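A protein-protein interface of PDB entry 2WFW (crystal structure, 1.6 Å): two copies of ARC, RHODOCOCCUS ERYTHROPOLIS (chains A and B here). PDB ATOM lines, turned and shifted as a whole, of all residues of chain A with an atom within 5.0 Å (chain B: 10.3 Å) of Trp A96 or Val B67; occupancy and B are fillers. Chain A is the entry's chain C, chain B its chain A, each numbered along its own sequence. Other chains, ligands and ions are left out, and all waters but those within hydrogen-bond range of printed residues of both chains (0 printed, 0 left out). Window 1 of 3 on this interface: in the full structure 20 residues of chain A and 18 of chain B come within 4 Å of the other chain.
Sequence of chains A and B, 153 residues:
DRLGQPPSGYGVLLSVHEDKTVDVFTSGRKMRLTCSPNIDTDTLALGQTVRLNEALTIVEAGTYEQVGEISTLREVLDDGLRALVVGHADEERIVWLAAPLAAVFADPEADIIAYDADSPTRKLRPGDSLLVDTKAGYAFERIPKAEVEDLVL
The side-chain carboxylate (OE1) of Glu B141 is in salt-bridge range of the guanidinium group (NH1) of Arg A82 (2.9 Å).
The backbone carbonyl oxygen (O) of Gln B66 lies within hydrogen-bond range of the guanidinium group (NH1) of Arg A82 (2.9 Å).
O of Gly B68 is in hydrogen-bond range of N of Ile A94, 2.8 Å away.
The backbone NH (N) of Ala A139 lies within hydrogen-bond range of the backbone carbonyl oxygen (O) of Trp A96 (2.9 Å).
The backbone NH (N) of Leu B131 lies within hydrogen-bond range of the backbone carbonyl oxygen (O) of Glu B141, at 2.9 Å.
The backbone carbonyl oxygen of Gly A137 sits at hydrogen-bond distance from the backbone NH of Trp A96.
Among the printed residues, pairs that only touch across the chains: Ile A94 with Gln B66, Ile A94 with Val B67, Ile A94 with Ile B70, Val A95 with Val B67, Trp A96 with Gln B66 and Trp A96 with Val B67.
Of the printed residues of chain B, Ile A94 touches Gln B66, Val B67, Gly B68 and Ile B70.
Of chain B, only Val B67 (3.8 Å) comes within 4 Å of Val A95.
Trp A96 touches just these residues of chain B: Gln B66 and Val B67.
Leu A97 touches none of the printed residues of chain B.
No residue of chain B comes within 4 Å of Gly A137.
No residue of chain B comes within 4 Å of Tyr A138.
Of the printed residues of chain A, Gln B66 touches Arg A82, Ile A94 and Trp A96.
Printed residues of chain A within 4 Å of Val B67: Ile A94 (3.3 Å), Val A95 (3.8 Å) and Trp A96 (3.4 Å).
Of the printed residues of chain A, Gly B68 touches Ile A94 (2.8 Å).
The nearest residue of chain A that does not touch Val B67 is Gly A137 (4.2 Å).
The nearest printed residue of chain A that does not touch Glu B141 is Ile A94 (6.6 Å).
Hydrophobic or aromatic side chains of chain B within 4 Å of the printed part of chain A: Val B67 and Ile B70.
Of the 11 printed residues of chain A, 4 touch a printed residue of chain B.
Printed residues of chain A that touch a printed residue of chain B: Arg A82, Ile A94, Val A95 and Trp A96.
Hydrophobic or aromatic side chains of chain A that line the printed part of chain B: Ile A94 and Trp A96.
2 positions are printed for both chains.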
ATOM      1  N   LEU A  81      24.651   8.834 -25.511  1.00  0.00           N
ATOM      2  CA  LEU A  81      23.376   8.083 -25.400  1.00  0.00           C
ATOM      3  C   LEU A  81      22.540   8.115 -26.669  1.00  0.00           C
ATOM      4  O   LEU A  81      21.669   7.260 -26.862  1.00  0.00           O
ATOM      5  CB  LEU A  81      22.522   8.645 -24.251  1.00  0.00           C
ATOM      6  CG  LEU A  81      23.122   8.696 -22.836  1.00  0.00           C
ATOM      7  CD1 LEU A  81      22.170   9.397 -21.867  1.00  0.00           C
ATOM      8  CD2 LEU A  81      23.496   7.316 -22.315  1.00  0.00           C
ATOM      9  N   ARG A  82      22.787   9.121 -27.510  1.00  0.00           N
ATOM     10  CA  ARG A  82      21.955   9.391 -28.691  1.00  0.00           C
ATOM     11  C   ARG A  82      22.866   9.580 -29.893  1.00  0.00           C
ATOM     12  O   ARG A  82      24.061   9.835 -29.740  1.00  0.00           O
ATOM     13  CB  ARG A  82      21.132  10.686 -28.486  1.00  0.00           C
ATOM     14  CG  ARG A  82      20.180  10.651 -27.296  1.00  0.00           C
ATOM     15  CD  ARG A  82      19.414  11.978 -27.136  1.00  0.00           C
ATOM     16  NE  ARG A  82      20.346  13.025 -26.737  1.00  0.00           N
ATOM     17  CZ  ARG A  82      20.121  14.338 -26.796  1.00  0.00           C
ATOM     18  NH1 ARG A  82      18.960  14.821 -27.254  1.00  0.00           N
ATOM     19  NH2 ARG A  82      21.063  15.171 -26.394  1.00  0.00           N
ATOM     20  N   ILE A  94      17.410  12.399 -34.551  1.00  0.00           N
ATOM     21  CA  ILE A  94      18.128  11.956 -33.355  1.00  0.00           C
ATOM     22  C   ILE A  94      17.465  10.672 -32.865  1.00  0.00           C
ATOM     23  O   ILE A  94      16.232  10.637 -32.761  1.00  0.00           O
ATOM     24  CB  ILE A  94      18.062  12.992 -32.191  1.00  0.00           C
ATOM     25  CG1 ILE A  94      18.633  14.344 -32.630  1.00  0.00           C
ATOM     26  CG2 ILE A  94      18.823  12.466 -30.967  1.00  0.00           C
ATOM     27  CD1 ILE A  94      19.998  14.215 -33.307  1.00  0.00           C
ATOM     28  N   VAL A  95      18.255   9.635 -32.595  1.00  0.00           N
ATOM     29  CA  VAL A  95      17.717   8.394 -32.004  1.00  0.00           C
ATOM     30  C   VAL A  95      18.521   8.004 -30.743  1.00  0.00           C
ATOM     31  O   VAL A  95      19.684   8.398 -30.585  1.00  0.00           O
ATOM     32  CB  VAL A  95      17.757   7.205 -33.018  1.00  0.00           C
ATOM     33  CG1 VAL A  95      16.862   7.506 -34.223  1.00  0.00           C
ATOM     34  CG2 VAL A  95      19.194   6.921 -33.478  1.00  0.00           C
ATOM     35  N   TRP A  96      17.918   7.223 -29.847  1.00  0.00           N
ATOM     36  CA  TRP A  96      18.662   6.631 -28.734  1.00  0.00           C
ATOM     37  C   TRP A  96      19.508   5.459 -29.248  1.00  0.00           C
ATOM     38  O   TRP A  96      19.073   4.752 -30.161  1.00  0.00           O
ATOM     39  CB  TRP A  96      17.703   6.024 -27.727  1.00  0.00           C
ATOM     40  CG  TRP A  96      16.788   7.013 -27.054  1.00  0.00           C
ATOM     41  CD1 TRP A  96      15.442   7.128 -27.238  1.00  0.00           C
ATOM     42  CD2 TRP A  96      17.144   7.968 -26.041  1.00  0.00           C
ATOM     43  NE1 TRP A  96      14.935   8.132 -26.425  1.00  0.00           N
ATOM     44  CE2 TRP A  96      15.963   8.657 -25.684  1.00  0.00           C
ATOM     45  CE3 TRP A  96      18.350   8.315 -25.404  1.00  0.00           C
ATOM     46  CZ2 TRP A  96      15.942   9.683 -24.718  1.00  0.00           C
ATOM     47  CZ3 TRP A  96      18.332   9.359 -24.440  1.00  0.00           C
ATOM     48  CH2 TRP A  96      17.127  10.013 -24.111  1.00  0.00           C
ATOM     49  N   LEU A  97      20.677   5.249 -28.645  1.00  0.00           N
ATOM     50  CA  LEU A  97      21.457   4.025 -28.907  1.00  0.00           C
ATOM     51  C   LEU A  97      21.006   2.863 -28.019  1.00  0.00           C
ATOM     52  O   LEU A  97      20.988   2.973 -26.777  1.00  0.00           O
ATOM     53  CB  LEU A  97      22.954   4.265 -28.665  1.00  0.00           C
ATOM     54  CG  LEU A  97      23.644   5.339 -29.509  1.00  0.00           C
ATOM     55  CD1 LEU A  97      25.099   5.463 -29.077  1.00  0.00           C
ATOM     56  CD2 LEU A  97      23.537   5.001 -30.998  1.00  0.00           C
ATOM     57  N   ALA A  98      20.655   1.735 -28.643  1.00  0.00           N
ATOM     58  CA  ALA A  98      20.362   0.521 -27.880  1.00  0.00           C
ATOM     59  C   ALA A  98      21.622   0.090 -27.117  1.00  0.00           C
ATOM     60  O   ALA A  98      22.745   0.400 -27.519  1.00  0.00           O
ATOM     61  CB  ALA A  98      19.898  -0.608 -28.799  1.00  0.00           C
ATOM     62  N   ALA A 136       9.949   4.491 -32.670  1.00  0.00           N
ATOM     63  CA  ALA A 136      10.354   4.284 -31.266  1.00  0.00           C
ATOM     64  C   ALA A 136      11.533   5.188 -30.929  1.00  0.00           C
ATOM     65  O   ALA A 136      11.769   5.505 -29.756  1.00  0.00           O
ATOM     66  CB  ALA A 136      10.693   2.803 -31.004  1.00  0.00           C
ATOM     67  N   GLY A 137      12.263   5.615 -31.958  1.00  0.00           N
ATOM     68  CA  GLY A 137      13.414   6.490 -31.767  1.00  0.00           C
ATOM     69  C   GLY A 137      14.677   5.799 -31.285  1.00  0.00           C
ATOM     70  O   GLY A 137      15.398   6.368 -30.464  1.00  0.00           O
ATOM     71  N   TYR A 138      14.942   4.602 -31.808  1.00  0.00           N
ATOM     72  CA  TYR A 138      16.108   3.794 -31.417  1.00  0.00           C
ATOM     73  C   TYR A 138      16.915   3.296 -32.616  1.00  0.00           C
ATOM     74  O   TYR A 138      16.356   3.034 -33.705  1.00  0.00           O
ATOM     75  CB  TYR A 138      15.700   2.553 -30.570  1.00  0.00           C
ATOM     76  CG  TYR A 138      15.912   2.773 -29.103  1.00  0.00           C
ATOM     77  CD1 TYR A 138      14.952   3.468 -28.324  1.00  0.00           C
ATOM     78  CD2 TYR A 138      17.111   2.394 -28.501  1.00  0.00           C
ATOM     79  CE1 TYR A 138      15.165   3.688 -26.972  1.00  0.00           C
ATOM     80  CE2 TYR A 138      17.348   2.621 -27.162  1.00  0.00           C
ATOM     81  CZ  TYR A 138      16.382   3.277 -26.395  1.00  0.00           C
ATOM     82  OH  TYR A 138      16.630   3.499 -25.066  1.00  0.00           O
ATOM     83  N   ALA A 139      18.227   3.184 -32.412  1.00  0.00           N
ATOM     84  CA  ALA A 139      19.080   2.383 -33.271  1.00  0.00           C
ATOM     85  C   ALA A 139      19.508   1.141 -32.507  1.00  0.00           C
ATOM     86  O   ALA A 139      19.883   1.243 -31.330  1.00  0.00           O
ATOM     87  CB  ALA A 139      20.317   3.198 -33.673  1.00  0.00           C
ATOM     88  N   VAL B  12       2.716  16.654 -25.175  1.00  0.00           N
ATOM     89  CA  VAL B  12       3.578  17.859 -25.145  1.00  0.00           C
ATOM     90  C   VAL B  12       2.752  19.033 -24.639  1.00  0.00           C
ATOM     91  O   VAL B  12       1.659  19.292 -25.190  1.00  0.00           O
ATOM     92  CB  VAL B  12       4.131  18.184 -26.557  1.00  0.00           C
ATOM     93  CG1 VAL B  12       4.851  19.563 -26.556  1.00  0.00           C
ATOM     94  CG2 VAL B  12       5.077  17.097 -27.034  1.00  0.00           C
ATOM     95  N   THR B  49       7.391  17.656 -21.891  1.00  0.00           N
ATOM     96  CA  THR B  49       6.548  16.473 -21.896  1.00  0.00           C
ATOM     97  C   THR B  49       5.787  16.350 -20.581  1.00  0.00           C
ATOM     98  O   THR B  49       6.355  16.533 -19.502  1.00  0.00           O
ATOM     99  CB  THR B  49       7.404  15.222 -22.133  1.00  0.00           C
ATOM    100  OG1 THR B  49       7.951  15.304 -23.446  1.00  0.00           O
ATOM    101  CG2 THR B  49       6.563  13.933 -22.037  1.00  0.00           C
ATOM    102  N   THR B  63      10.637  16.541 -18.841  1.00  0.00           N
ATOM    103  CA  THR B  63      11.635  17.276 -19.608  1.00  0.00           C
ATOM    104  C   THR B  63      11.151  17.464 -21.037  1.00  0.00           C
ATOM    105  O   THR B  63      10.067  16.987 -21.408  1.00  0.00           O
ATOM    106  CB  THR B  63      12.971  16.454 -19.676  1.00  0.00           C
ATOM    107  OG1 THR B  63      12.712  15.177 -20.271  1.00  0.00           O
ATOM    108  CG2 THR B  63      13.589  16.251 -18.303  1.00  0.00           C
ATOM    109  N   TYR B  64      11.969  18.087 -21.877  1.00  0.00           N
ATOM    110  CA  TYR B  64      11.640  18.194 -23.298  1.00  0.00           C
ATOM    111  C   TYR B  64      11.996  16.900 -24.016  1.00  0.00           C
ATOM    112  O   TYR B  64      12.889  16.183 -23.564  1.00  0.00           O
ATOM    113  CB  TYR B  64      12.398  19.347 -23.933  1.00  0.00           C
ATOM    114  CG  TYR B  64      12.132  20.656 -23.216  1.00  0.00           C
ATOM    115  CD1 TYR B  64      10.908  21.322 -23.359  1.00  0.00           C
ATOM    116  CD2 TYR B  64      13.096  21.214 -22.385  1.00  0.00           C
ATOM    117  CE1 TYR B  64      10.638  22.525 -22.688  1.00  0.00           C
ATOM    118  CE2 TYR B  64      12.859  22.417 -21.712  1.00  0.00           C
ATOM    119  CZ  TYR B  64      11.631  23.064 -21.854  1.00  0.00           C
ATOM    120  OH  TYR B  64      11.438  24.257 -21.182  1.00  0.00           O
ATOM    121  N   GLU B  65      11.315  16.635 -25.133  1.00  0.00           N
ATOM    122  CA  GLU B  65      11.681  15.504 -26.000  1.00  0.00           C
ATOM    123  C   GLU B  65      13.161  15.536 -26.327  1.00  0.00           C
ATOM    124  O   GLU B  65      13.753  16.599 -26.510  1.00  0.00           O
ATOM    125  CB  GLU B  65      10.875  15.497 -27.300  1.00  0.00           C
ATOM    126  CG  GLU B  65       9.386  15.306 -27.150  1.00  0.00           C
ATOM    127  CD  GLU B  65       8.660  15.474 -28.511  1.00  0.00           C
ATOM    128  OE1 GLU B  65       9.295  15.290 -29.566  1.00  0.00           O
ATOM    129  OE2 GLU B  65       7.483  15.796 -28.530  1.00  0.00           O
ATOM    130  N   GLN B  66      13.744  14.352 -26.423  1.00  0.00           N
ATOM    131  CA  GLN B  66      15.187  14.223 -26.668  1.00  0.00           C
ATOM    132  C   GLN B  66      15.537  13.464 -27.963  1.00  0.00           C
ATOM    133  O   GLN B  66      16.711  13.390 -28.349  1.00  0.00           O
ATOM    134  CB  GLN B  66      15.854  13.558 -25.475  1.00  0.00           C
ATOM    135  CG  GLN B  66      16.026  14.498 -24.294  1.00  0.00           C
ATOM    136  CD  GLN B  66      16.662  13.820 -23.134  1.00  0.00           C
ATOM    137  OE1 GLN B  66      16.123  12.846 -22.601  1.00  0.00           O
ATOM    138  NE2 GLN B  66      17.827  14.316 -22.723  1.00  0.00           N
ATOM    139  N   VAL B  67      14.531  12.886 -28.618  1.00  0.00           N
ATOM    140  CA  VAL B  67      14.742  12.209 -29.896  1.00  0.00           C
ATOM    141  C   VAL B  67      13.665  12.658 -30.846  1.00  0.00           C
ATOM    142  O   VAL B  67      12.626  13.158 -30.404  1.00  0.00           O
ATOM    143  CB  VAL B  67      14.760  10.641 -29.758  1.00  0.00           C
ATOM    144  CG1 VAL B  67      15.964  10.212 -28.943  1.00  0.00           C
ATOM    145  CG2 VAL B  67      13.461  10.108 -29.160  1.00  0.00           C
ATOM    146  N   GLY B  68      13.931  12.487 -32.131  1.00  0.00           N
ATOM    147  CA  GLY B  68      13.015  12.902 -33.178  1.00  0.00           C
ATOM    148  C   GLY B  68      13.655  13.639 -34.344  1.00  0.00           C
ATOM    149  O   GLY B  68      14.856  13.545 -34.602  1.00  0.00           O
ATOM    150  N   GLU B  69      12.817  14.371 -35.066  1.00  0.00           N
ATOM    151  CA  GLU B  69      13.199  15.014 -36.314  1.00  0.00           C
ATOM    152  C   GLU B  69      14.185  16.158 -36.108  1.00  0.00           C
ATOM    153  O   GLU B  69      14.103  16.869 -35.121  1.00  0.00           O
ATOM    154  CB  GLU B  69      11.920  15.575 -36.954  1.00  0.00           C
ATOM    155  CG  GLU B  69      12.113  16.128 -38.328  1.00  0.00           C
ATOM    156  CD  GLU B  69      10.799  16.464 -39.031  1.00  0.00           C
ATOM    157  OE1 GLU B  69       9.703  16.090 -38.537  1.00  0.00           O
ATOM    158  OE2 GLU B  69      10.880  17.135 -40.090  1.00  0.00           O
ATOM    159  N   ILE B  70      15.074  16.363 -37.074  1.00  0.00           N
ATOM    160  CA  ILE B  70      15.946  17.529 -37.073  1.00  0.00           C
ATOM    161  C   ILE B  70      15.542  18.474 -38.187  1.00  0.00           C
ATOM    162  O   ILE B  70      15.239  18.039 -39.301  1.00  0.00           O
ATOM    163  CB  ILE B  70      17.425  17.096 -37.271  1.00  0.00           C
ATOM    164  CG1 ILE B  70      17.930  16.383 -36.009  1.00  0.00           C
ATOM    165  CG2 ILE B  70      18.286  18.276 -37.675  1.00  0.00           C
ATOM    166  CD1 ILE B  70      18.102  17.314 -34.849  1.00  0.00           C
ATOM    167  N   SER B  71      15.510  19.766 -37.855  1.00  0.00           N
ATOM    168  CA  SER B  71      15.220  20.819 -38.809  1.00  0.00           C
ATOM    169  C   SER B  71      16.252  21.926 -38.667  1.00  0.00           C
ATOM    170  O   SER B  71      16.920  21.999 -37.649  1.00  0.00           O
ATOM    171  CB  SER B  71      13.846  21.388 -38.541  1.00  0.00           C
ATOM    172  OG  SER B  71      13.346  21.934 -39.730  1.00  0.00           O
ATOM    173  N   LEU B 130      18.141  22.008 -35.172  1.00  0.00           N
ATOM    174  CA  LEU B 130      17.271  21.917 -34.019  1.00  0.00           C
ATOM    175  C   LEU B 130      16.487  20.614 -34.007  1.00  0.00           C
ATOM    176  O   LEU B 130      15.951  20.208 -35.031  1.00  0.00           O
ATOM    177  CB  LEU B 130      16.269  23.081 -34.000  1.00  0.00           C
ATOM    178  CG  LEU B 130      16.824  24.509 -34.049  1.00  0.00           C
ATOM    179  CD1 LEU B 130      15.700  25.560 -34.023  1.00  0.00           C
ATOM    180  CD2 LEU B 130      17.835  24.705 -32.894  1.00  0.00           C
ATOM    181  N   LEU B 131      16.421  19.989 -32.835  1.00  0.00           N
ATOM    182  CA  LEU B 131      15.510  18.892 -32.567  1.00  0.00           C
ATOM    183  C   LEU B 131      14.097  19.486 -32.477  1.00  0.00           C
ATOM    184  O   LEU B 131      13.852  20.419 -31.695  1.00  0.00           O
ATOM    185  CB  LEU B 131      15.855  18.257 -31.225  1.00  0.00           C
ATOM    186  CG  LEU B 131      14.924  17.098 -30.804  1.00  0.00           C
ATOM    187  CD1 LEU B 131      14.879  15.956 -31.844  1.00  0.00           C
ATOM    188  CD2 LEU B 131      15.354  16.571 -29.457  1.00  0.00           C
ATOM    189  N   VAL B 132      13.200  18.967 -33.300  1.00  0.00           N
ATOM    190  CA  VAL B 132      11.815  19.482 -33.410  1.00  0.00           C
ATOM    191  C   VAL B 132      10.802  18.346 -33.322  1.00  0.00           C
ATOM    192  O   VAL B 132      11.108  17.162 -33.574  1.00  0.00           O
ATOM    193  CB  VAL B 132      11.572  20.309 -34.706  1.00  0.00           C
ATOM    194  CG1 VAL B 132      12.481  21.538 -34.751  1.00  0.00           C
ATOM    195  CG2 VAL B 132      11.771  19.447 -35.952  1.00  0.00           C
ATOM    196  N   ASP B 133       9.592  18.725 -32.923  1.00  0.00           N
ATOM    197  CA  ASP B 133       8.427  17.871 -33.035  1.00  0.00           C
ATOM    198  C   ASP B 133       7.470  18.690 -33.883  1.00  0.00           C
ATOM    199  O   ASP B 133       6.860  19.651 -33.387  1.00  0.00           O
ATOM    200  CB  ASP B 133       7.852  17.549 -31.650  1.00  0.00           C
ATOM    201  CG  ASP B 133       6.622  16.650 -31.709  1.00  0.00           C
ATOM    202  OD1 ASP B 133       5.908  16.606 -32.752  1.00  0.00           O
ATOM    203  OD2 ASP B 133       6.332  15.944 -30.698  1.00  0.00           O
ATOM    204  N   THR B 134       7.375  18.351 -35.165  1.00  0.00           N
ATOM    205  CA  THR B 134       6.576  19.165 -36.087  1.00  0.00           C
ATOM    206  C   THR B 134       5.071  18.972 -35.896  1.00  0.00           C
ATOM    207  O   THR B 134       4.297  19.828 -36.284  1.00  0.00           O
ATOM    208  CB  THR B 134       6.931  18.888 -37.585  1.00  0.00           C
ATOM    209  OG1 THR B 134       6.595  17.525 -37.901  1.00  0.00           O
ATOM    210  CG2 THR B 134       8.410  19.153 -37.853  1.00  0.00           C
ATOM    211  N   TYR B 138       6.919  22.314 -31.970  1.00  0.00           N
ATOM    212  CA  TYR B 138       7.954  22.765 -31.022  1.00  0.00           C
ATOM    213  C   TYR B 138       9.377  22.475 -31.489  1.00  0.00           C
ATOM    214  O   TYR B 138       9.621  21.456 -32.142  1.00  0.00           O
ATOM    215  CB  TYR B 138       7.789  22.106 -29.619  1.00  0.00           C
ATOM    216  CG  TYR B 138       7.257  23.098 -28.629  1.00  0.00           C
ATOM    217  CD1 TYR B 138       5.881  23.244 -28.417  1.00  0.00           C
ATOM    218  CD2 TYR B 138       8.140  23.967 -27.963  1.00  0.00           C
ATOM    219  CE1 TYR B 138       5.398  24.228 -27.534  1.00  0.00           C
ATOM    220  CE2 TYR B 138       7.666  24.953 -27.100  1.00  0.00           C
ATOM    221  CZ  TYR B 138       6.305  25.078 -26.884  1.00  0.00           C
ATOM    222  OH  TYR B 138       5.869  26.082 -26.034  1.00  0.00           O
ATOM    223  N   ALA B 139      10.290  23.381 -31.137  1.00  0.00           N
ATOM    224  CA  ALA B 139      11.729  23.133 -31.239  1.00  0.00           C
ATOM    225  C   ALA B 139      12.268  23.085 -29.809  1.00  0.00           C
ATOM    226  O   ALA B 139      11.968  23.987 -28.997  1.00  0.00           O
ATOM    227  CB  ALA B 139      12.418  24.247 -32.024  1.00  0.00           C
ATOM    228  N   PHE B 140      13.125  22.103 -29.524  1.00  0.00           N
ATOM    229  CA  PHE B 140      13.527  21.827 -28.140  1.00  0.00           C
ATOM    230  C   PHE B 140      14.989  22.052 -27.788  1.00  0.00           C
ATOM    231  O   PHE B 140      15.284  22.425 -26.660  1.00  0.00           O
ATOM    232  CB  PHE B 140      13.265  20.363 -27.797  1.00  0.00           C
ATOM    233  CG  PHE B 140      11.832  19.950 -27.957  1.00  0.00           C
ATOM    234  CD1 PHE B 140      11.486  19.026 -28.935  1.00  0.00           C
ATOM    235  CD2 PHE B 140      10.836  20.428 -27.090  1.00  0.00           C
ATOM    236  CE1 PHE B 140      10.162  18.621 -29.079  1.00  0.00           C
ATOM    237  CE2 PHE B 140       9.507  20.004 -27.222  1.00  0.00           C
ATOM    238  CZ  PHE B 140       9.168  19.115 -28.212  1.00  0.00           C
ATOM    239  N   GLU B 141      15.873  21.731 -28.738  1.00  0.00           N
ATOM    240  CA  GLU B 141      17.300  21.563 -28.454  1.00  0.00           C
ATOM    241  C   GLU B 141      18.124  21.866 -29.697  1.00  0.00           C
ATOM    242  O   GLU B 141      17.718  21.550 -30.811  1.00  0.00           O
ATOM    243  CB  GLU B 141      17.545  20.107 -28.000  1.00  0.00           C
ATOM    244  CG  GLU B 141      18.948  19.817 -27.468  1.00  0.00           C
ATOM    245  CD  GLU B 141      19.184  18.357 -27.039  1.00  0.00           C
ATOM    246  OE1 GLU B 141      18.219  17.574 -26.904  1.00  0.00           O
ATOM    247  OE2 GLU B 141      20.365  18.025 -26.804  1.00  0.00           O
ATOM    248  N   ILE B 143      21.507  20.958 -31.792  1.00  0.00           N
ATOM    249  CA  ILE B 143      22.332  19.780 -32.007  1.00  0.00           C
ATOM    250  C   ILE B 143      23.576  20.269 -32.734  1.00  0.00           C
ATOM    251  O   ILE B 143      23.461  20.836 -33.826  1.00  0.00           O
ATOM    252  CB  ILE B 143      21.569  18.749 -32.887  1.00  0.00           C
ATOM    253  CG1 ILE B 143      20.200  18.431 -32.262  1.00  0.00           C
ATOM    254  CG2 ILE B 143      22.394  17.468 -33.124  1.00  0.00           C
ATOM    255  CD1 ILE B 143      20.269  17.739 -30.876  1.00  0.00           C
